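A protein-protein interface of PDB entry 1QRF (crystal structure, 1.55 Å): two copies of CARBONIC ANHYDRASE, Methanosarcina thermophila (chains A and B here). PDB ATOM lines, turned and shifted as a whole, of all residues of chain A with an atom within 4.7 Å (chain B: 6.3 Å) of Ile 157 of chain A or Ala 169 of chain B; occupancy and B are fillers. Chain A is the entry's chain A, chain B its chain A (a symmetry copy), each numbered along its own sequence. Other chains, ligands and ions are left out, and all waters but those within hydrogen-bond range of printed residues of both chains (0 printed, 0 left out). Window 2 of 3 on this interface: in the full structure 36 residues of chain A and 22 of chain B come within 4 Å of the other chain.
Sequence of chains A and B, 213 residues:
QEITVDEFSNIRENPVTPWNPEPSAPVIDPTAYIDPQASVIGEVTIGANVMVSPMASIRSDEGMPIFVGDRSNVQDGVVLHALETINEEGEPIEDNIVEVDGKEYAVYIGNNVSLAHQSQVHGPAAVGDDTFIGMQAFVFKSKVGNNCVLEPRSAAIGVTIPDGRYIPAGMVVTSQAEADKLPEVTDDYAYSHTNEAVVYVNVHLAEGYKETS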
ATOM      1  N   PHE A 138       5.667  14.433  -4.728  1.00  0.00           N
ATOM      2  CA  PHE A 138       5.626  13.007  -5.024  1.00  0.00           C
ATOM      3  C   PHE A 138       7.026  12.467  -5.283  1.00  0.00           C
ATOM      4  O   PHE A 138       7.754  13.107  -6.025  1.00  0.00           O
ATOM      5  CB  PHE A 138       4.716  12.733  -6.233  1.00  0.00           C
ATOM      6  CG  PHE A 138       4.599  11.297  -6.630  1.00  0.00           C
ATOM      7  CD1 PHE A 138       4.011  10.336  -5.810  1.00  0.00           C
ATOM      8  CD2 PHE A 138       4.987  10.916  -7.917  1.00  0.00           C
ATOM      9  CE1 PHE A 138       3.868   9.014  -6.241  1.00  0.00           C
ATOM     10  CE2 PHE A 138       4.860   9.612  -8.320  1.00  0.00           C
ATOM     11  CZ  PHE A 138       4.325   8.635  -7.503  1.00  0.00           C
ATOM     12  N   PHE A 140       8.836   8.684  -6.324  1.00  0.00           N
ATOM     13  CA  PHE A 140       8.614   7.296  -6.670  1.00  0.00           C
ATOM     14  C   PHE A 140       9.776   6.733  -7.500  1.00  0.00           C
ATOM     15  O   PHE A 140      10.223   7.465  -8.358  1.00  0.00           O
ATOM     16  CB  PHE A 140       7.349   7.256  -7.545  1.00  0.00           C
ATOM     17  CG  PHE A 140       6.972   5.916  -8.108  1.00  0.00           C
ATOM     18  CD1 PHE A 140       7.007   4.750  -7.359  1.00  0.00           C
ATOM     19  CD2 PHE A 140       6.530   5.851  -9.417  1.00  0.00           C
ATOM     20  CE1 PHE A 140       6.584   3.518  -7.931  1.00  0.00           C
ATOM     21  CE2 PHE A 140       6.117   4.659  -9.985  1.00  0.00           C
ATOM     22  CZ  PHE A 140       6.163   3.497  -9.240  1.00  0.00           C
ATOM     23  N   LYS A 141      10.258   5.540  -7.145  1.00  0.00           N
ATOM     24  CA  LYS A 141      11.404   4.977  -7.869  1.00  0.00           C
ATOM     25  C   LYS A 141      12.530   5.987  -7.989  1.00  0.00           C
ATOM     26  O   LYS A 141      13.181   6.181  -9.020  1.00  0.00           O
ATOM     27  CB  LYS A 141      10.996   4.490  -9.262  1.00  0.00           C
ATOM     28  CG  LYS A 141       9.957   3.384  -9.262  1.00  0.00           C
ATOM     29  CD  LYS A 141       9.673   2.942 -10.704  1.00  0.00           C
ATOM     30  CE  LYS A 141      10.732   1.981 -11.210  1.00  0.00           C
ATOM     31  NZ  LYS A 141      10.327   1.484 -12.561  1.00  0.00           N
ATOM     32  N   SER A 142      12.833   6.655  -6.866  1.00  0.00           N
ATOM     33  CA  SER A 142      13.867   7.688  -6.843  1.00  0.00           C
ATOM     34  C   SER A 142      14.598   7.661  -5.508  1.00  0.00           C
ATOM     35  O   SER A 142      14.148   7.173  -4.466  1.00  0.00           O
ATOM     36  CB  SER A 142      13.228   9.093  -6.985  1.00  0.00           C
ATOM     37  OG  SER A 142      12.652   9.261  -8.277  1.00  0.00           O
ATOM     38  N   ALA A 155       7.856  16.771  -8.214  1.00  0.00           N
ATOM     39  CA  ALA A 155       7.881  15.306  -8.212  1.00  0.00           C
ATOM     40  C   ALA A 155       9.226  14.775  -8.704  1.00  0.00           C
ATOM     41  O   ALA A 155       9.830  15.470  -9.550  1.00  0.00           O
ATOM     42  CB  ALA A 155       6.788  14.690  -9.116  1.00  0.00           C
ATOM     43  N   ALA A 156       9.654  13.689  -8.156  1.00  0.00           N
ATOM     44  CA  ALA A 156      10.878  12.987  -8.601  1.00  0.00           C
ATOM     45  C   ALA A 156      10.503  11.559  -8.936  1.00  0.00           C
ATOM     46  O   ALA A 156      10.043  10.786  -8.065  1.00  0.00           O
ATOM     47  CB  ALA A 156      11.963  13.020  -7.572  1.00  0.00           C
ATOM     48  N   ILE A 157      10.579  11.137 -10.198  1.00  0.00           N
ATOM     49  CA  ILE A 157      10.197   9.792 -10.600  1.00  0.00           C
ATOM     50  C   ILE A 157      11.316   9.159 -11.446  1.00  0.00           C
ATOM     51  O   ILE A 157      11.646   9.735 -12.471  1.00  0.00           O
ATOM     52  CB  ILE A 157       8.952   9.824 -11.498  1.00  0.00           C
ATOM     53  CG1 ILE A 157       7.746  10.494 -10.840  1.00  0.00           C
ATOM     54  CG2 ILE A 157       8.571   8.410 -11.977  1.00  0.00           C
ATOM     55  CD1 ILE A 157       6.529  10.759 -11.685  1.00  0.00           C
ATOM     56  N   GLY A 158      11.803   8.024 -11.008  1.00  0.00           N
ATOM     57  CA  GLY A 158      12.846   7.280 -11.739  1.00  0.00           C
ATOM     58  C   GLY A 158      14.208   7.920 -11.702  1.00  0.00           C
ATOM     59  O   GLY A 158      15.063   7.568 -12.553  1.00  0.00           O
ATOM     60  N   VAL A 159      14.500   8.830 -10.767  1.00  0.00           N
ATOM     61  CA  VAL A 159      15.779   9.553 -10.754  1.00  0.00           C
ATOM     62  C   VAL A 159      16.488   9.603  -9.415  1.00  0.00           C
ATOM     63  O   VAL A 159      15.986   9.275  -8.340  1.00  0.00           O
ATOM     64  CB  VAL A 159      15.436  11.017 -11.134  1.00  0.00           C
ATOM     65  CG1 VAL A 159      14.932  11.153 -12.547  1.00  0.00           C
ATOM     66  CG2 VAL A 159      14.399  11.603 -10.148  1.00  0.00           C
ATOM     67  N   VAL A 172       7.926  18.350 -12.565  1.00  0.00           N
ATOM     68  CA  VAL A 172       7.947  16.857 -12.517  1.00  0.00           C
ATOM     69  C   VAL A 172       9.222  16.355 -13.150  1.00  0.00           C
ATOM     70  O   VAL A 172       9.425  16.466 -14.376  1.00  0.00           O
ATOM     71  CB  VAL A 172       6.701  16.311 -13.220  1.00  0.00           C
ATOM     72  CG1 VAL A 172       6.744  14.793 -13.235  1.00  0.00           C
ATOM     73  CG2 VAL A 172       5.419  16.778 -12.532  1.00  0.00           C
ATOM     74  N   VAL A 173      10.155  15.869 -12.362  1.00  0.00           N
ATOM     75  CA  VAL A 173      11.457  15.420 -12.821  1.00  0.00           C
ATOM     76  C   VAL A 173      11.406  13.919 -13.069  1.00  0.00           C
ATOM     77  O   VAL A 173      11.210  13.115 -12.173  1.00  0.00           O
ATOM     78  CB  VAL A 173      12.566  15.772 -11.837  1.00  0.00           C
ATOM     79  CG1 VAL A 173      13.932  15.257 -12.308  1.00  0.00           C
ATOM     80  CG2 VAL A 173      12.549  17.283 -11.626  1.00  0.00           C
ATOM     81  N   THR A 174      11.570  13.548 -14.333  1.00  0.00           N
ATOM     82  CA  THR A 174      11.507  12.161 -14.758  1.00  0.00           C
ATOM     83  C   THR A 174      12.784  11.656 -15.437  1.00  0.00           C
ATOM     84  O   THR A 174      12.831  10.483 -15.794  1.00  0.00           O
ATOM     85  CB  THR A 174      10.373  11.911 -15.771  1.00  0.00           C
ATOM     86  OG1 THR A 174      10.499  12.778 -16.902  1.00  0.00           O
ATOM     87  CG2 THR A 174       9.019  12.166 -15.121  1.00  0.00           C
ATOM     88  N   LEU B 150      -2.826   6.207 -16.724  1.00  0.00           N
ATOM     89  CA  LEU B 150      -2.657   7.592 -16.405  1.00  0.00           C
ATOM     90  C   LEU B 150      -1.418   7.599 -15.492  1.00  0.00           C
ATOM     91  O   LEU B 150      -1.478   7.010 -14.388  1.00  0.00           O
ATOM     92  CB  LEU B 150      -3.856   8.275 -15.728  1.00  0.00           C
ATOM     93  CG  LEU B 150      -4.762   9.064 -16.675  1.00  0.00           C
ATOM     94  CD1 LEU B 150      -5.496   8.099 -17.580  1.00  0.00           C
ATOM     95  CD2 LEU B 150      -5.727   9.967 -15.931  1.00  0.00           C
ATOM     96  N   GLU B 151      -0.288   8.106 -15.938  1.00  0.00           N
ATOM     97  CA  GLU B 151       0.904   8.133 -15.074  1.00  0.00           C
ATOM     98  C   GLU B 151       0.658   9.007 -13.849  1.00  0.00           C
ATOM     99  O   GLU B 151      -0.294   9.778 -13.806  1.00  0.00           O
ATOM    100  CB  GLU B 151       2.133   8.616 -15.864  1.00  0.00           C
ATOM    101  CG  GLU B 151       2.462   7.628 -16.982  1.00  0.00           C
ATOM    102  CD  GLU B 151       3.788   7.982 -17.665  1.00  0.00           C
ATOM    103  OE1 GLU B 151       4.531   8.832 -17.164  1.00  0.00           O
ATOM    104  OE2 GLU B 151       4.017   7.340 -18.736  1.00  0.00           O
ATOM    105  N   PRO B 152       1.491   8.889 -12.847  1.00  0.00           N
ATOM    106  CA  PRO B 152       1.341   9.676 -11.632  1.00  0.00           C
ATOM    107  C   PRO B 152       1.217  11.150 -11.929  1.00  0.00           C
ATOM    108  O   PRO B 152       1.880  11.704 -12.829  1.00  0.00           O
ATOM    109  CB  PRO B 152       2.604   9.402 -10.778  1.00  0.00           C
ATOM    110  CG  PRO B 152       2.913   8.000 -11.230  1.00  0.00           C
ATOM    111  CD  PRO B 152       2.606   7.949 -12.747  1.00  0.00           C
ATOM    112  N   ARG B 153       0.291  11.875 -11.318  1.00  0.00           N
ATOM    113  CA  ARG B 153       0.055  13.292 -11.496  1.00  0.00           C
ATOM    114  C   ARG B 153      -0.476  13.704 -12.865  1.00  0.00           C
ATOM    115  O   ARG B 153      -0.482  14.928 -13.109  1.00  0.00           O
ATOM    116  CB  ARG B 153       1.367  14.090 -11.342  1.00  0.00           C
ATOM    117  CG  ARG B 153       1.687  14.408  -9.933  1.00  0.00           C
ATOM    118  CD  ARG B 153       0.879  15.571  -9.344  1.00  0.00           C
ATOM    119  NE  ARG B 153       1.589  15.761  -8.076  1.00  0.00           N
ATOM    120  CZ  ARG B 153       2.800  16.318  -7.988  1.00  0.00           C
ATOM    121  NH1 ARG B 153       3.440  16.823  -9.042  1.00  0.00           N
ATOM    122  NH2 ARG B 153       3.256  16.332  -6.763  1.00  0.00           N
ATOM    123  N   SER B 154      -0.929  12.780 -13.670  1.00  0.00           N
ATOM    124  CA  SER B 154      -1.565  13.173 -14.950  1.00  0.00           C
ATOM    125  C   SER B 154      -3.025  13.516 -14.641  1.00  0.00           C
ATOM    126  O   SER B 154      -3.552  13.180 -13.532  1.00  0.00           O
ATOM    127  CB  SER B 154      -1.421  12.053 -15.930  1.00  0.00           C
ATOM    128  OG  SER B 154      -2.089  10.841 -15.584  1.00  0.00           O
ATOM    129  N   ILE B 167      -1.253   8.695 -20.507  1.00  0.00           N
ATOM    130  CA  ILE B 167      -1.027  10.098 -20.260  1.00  0.00           C
ATOM    131  C   ILE B 167       0.241  10.245 -19.463  1.00  0.00           C
ATOM    132  O   ILE B 167       0.410   9.836 -18.285  1.00  0.00           O
ATOM    133  CB  ILE B 167      -2.167  10.807 -19.486  1.00  0.00           C
ATOM    134  CG1 ILE B 167      -3.547  10.553 -20.109  1.00  0.00           C
ATOM    135  CG2 ILE B 167      -1.854  12.314 -19.404  1.00  0.00           C
ATOM    136  CD1 ILE B 167      -4.686  11.386 -19.497  1.00  0.00           C
ATOM    137  N   PRO B 168       1.288  10.830 -20.030  1.00  0.00           N
ATOM    138  CA  PRO B 168       2.555  11.066 -19.380  1.00  0.00           C
ATOM    139  C   PRO B 168       2.456  11.753 -18.022  1.00  0.00           C
ATOM    140  O   PRO B 168       1.616  12.628 -17.804  1.00  0.00           O
ATOM    141  CB  PRO B 168       3.363  11.954 -20.384  1.00  0.00           C
ATOM    142  CG  PRO B 168       2.682  11.618 -21.665  1.00  0.00           C
ATOM    143  CD  PRO B 168       1.220  11.298 -21.458  1.00  0.00           C
ATOM    144  N   ALA B 169       3.311  11.410 -17.041  1.00  0.00           N
ATOM    145  CA  ALA B 169       3.315  12.015 -15.724  1.00  0.00           C
ATOM    146  C   ALA B 169       3.236  13.530 -15.760  1.00  0.00           C
ATOM    147  O   ALA B 169       3.943  14.214 -16.542  1.00  0.00           O
ATOM    148  CB  ALA B 169       4.595  11.640 -14.972  1.00  0.00           C
ATOM    149  N   GLY B 170       2.332  14.108 -14.972  1.00  0.00           N
ATOM    150  CA  GLY B 170       2.194  15.555 -14.851  1.00  0.00           C
ATOM    151  C   GLY B 170       1.368  16.217 -15.912  1.00  0.00           C
ATOM    152  O   GLY B 170       0.974  17.400 -15.714  1.00  0.00           O
ATOM    153  N   MET B 171       1.012  15.543 -16.999  1.00  0.00           N
ATOM    154  CA  MET B 171       0.249  16.176 -18.063  1.00  0.00           C
ATOM    155  C   MET B 171      -1.239  16.325 -17.763  1.00  0.00           C
ATOM    156  O   MET B 171      -1.906  15.353 -17.375  1.00  0.00           O
ATOM    157  CB  MET B 171       0.474  15.381 -19.363  1.00  0.00           C
ATOM    158  CG  MET B 171      -0.143  16.102 -20.567  1.00  0.00           C
ATOM    159  SD  MET B 171      -0.040  15.031 -22.041  1.00  0.00           S
ATOM    160  CE  MET B 171       1.754  15.045 -22.149  1.00  0.00           C
ATOM    161  N   TYR B 191       5.026   1.533 -18.230  1.00  0.00           N
ATOM    162  CA  TYR B 191       3.897   1.082 -17.389  1.00  0.00           C
ATOM    163  C   TYR B 191       3.021   0.060 -18.081  1.00  0.00           C
ATOM    164  O   TYR B 191       1.883  -0.200 -17.639  1.00  0.00           O
ATOM    165  CB  TYR B 191       3.031   2.298 -17.032  1.00  0.00           C
ATOM    166  CG  TYR B 191       3.658   3.315 -16.131  1.00  0.00           C
ATOM    167  CD1 TYR B 191       4.517   4.311 -16.548  1.00  0.00           C
ATOM    168  CD2 TYR B 191       3.344   3.328 -14.754  1.00  0.00           C
ATOM    169  CE1 TYR B 191       5.089   5.241 -15.721  1.00  0.00           C
ATOM    170  CE2 TYR B 191       3.906   4.236 -13.920  1.00  0.00           C
ATOM    171  CZ  TYR B 191       4.774   5.212 -14.362  1.00  0.00           C
ATOM    172  OH  TYR B 191       5.285   6.125 -13.500  1.00  0.00           O
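Pro 152 of chain B touches Phe 138 of chain A (CB to CE2, 3.3 Å).
Phe 138 of chain A touches Arg 153 of chain B (N to NH2, 3.7 Å).
Tyr 191 of chain B touches Phe 140 of chain A (OH to CE2, 3.9 Å).
CB of Ala 155 of chain A touches NH1 of Arg 153 of chain B, at 3.97 Å.
Ala 169 of chain B touches Ile 157 of chain A.
Of the 12 printed residues of chain A, 4 touch a printed residue of chain B.
Along chain A the printed residues that touch a printed residue of chain B span positions 138 to 157.
No position is printed for both chains.
The backbone NH (N) of Gly 158 of chain A lies within hydrogen-bond range of the backbone carbonyl oxygen (O) of Phe 140 of chain A (3.1 Å).
The backbone carbonyl oxygen (O) of Ala 156 of chain A sits at hydrogen-bond distance from the backbone NH (N) of Phe 140 of chain A, 3.0 Å away.
OE1 of Glu 151 of chain B is in hydrogen-bond range of N of Ala 169 of chain B (2.9 Å).
The backbone carbonyl oxygen (O) of Pro 152 of chain B lies within hydrogen-bond range of the backbone NH (N) of Gly 170 of chain B (3.3 Å).
The backbone carbonyl oxygen (O) of Ala 155 of chain A lies within hydrogen-bond range of the backbone NH (N) of Val 173 of chain A (2.9 Å).
The backbone carbonyl oxygen (O) of Arg 153 of chain B sits close to the backbone NH (N) of Gly 170 of chain B (3.5 Å).
Ile 157 of chain A touches just one residue of chain B: Ala 169.
Ala 169 of chain B touches just one residue of chain A: Ile 157.
Of the printed residues of chain A, Tyr 191 of chain B touches Phe 140.
Of the printed residues of chain B, Ala 155 of chain A touches Arg 153.
Of the printed residues of chain B, Phe 138 of chain A touches Pro 152 and Arg 153.
Printed residues of chain A within 4 Å of Arg 153 of chain B: Phe 138 (3.7 Å) and Ala 155 (3.97 Å).
Ile 167 of chain B touches none of the printed residues of chain A.
Thr 174 of chain A touches none of the printed residues of chain B.
The nearest residue of chain B that does not touch Ile 157 of chain A is Pro 152 of chain B (4.3 Å).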
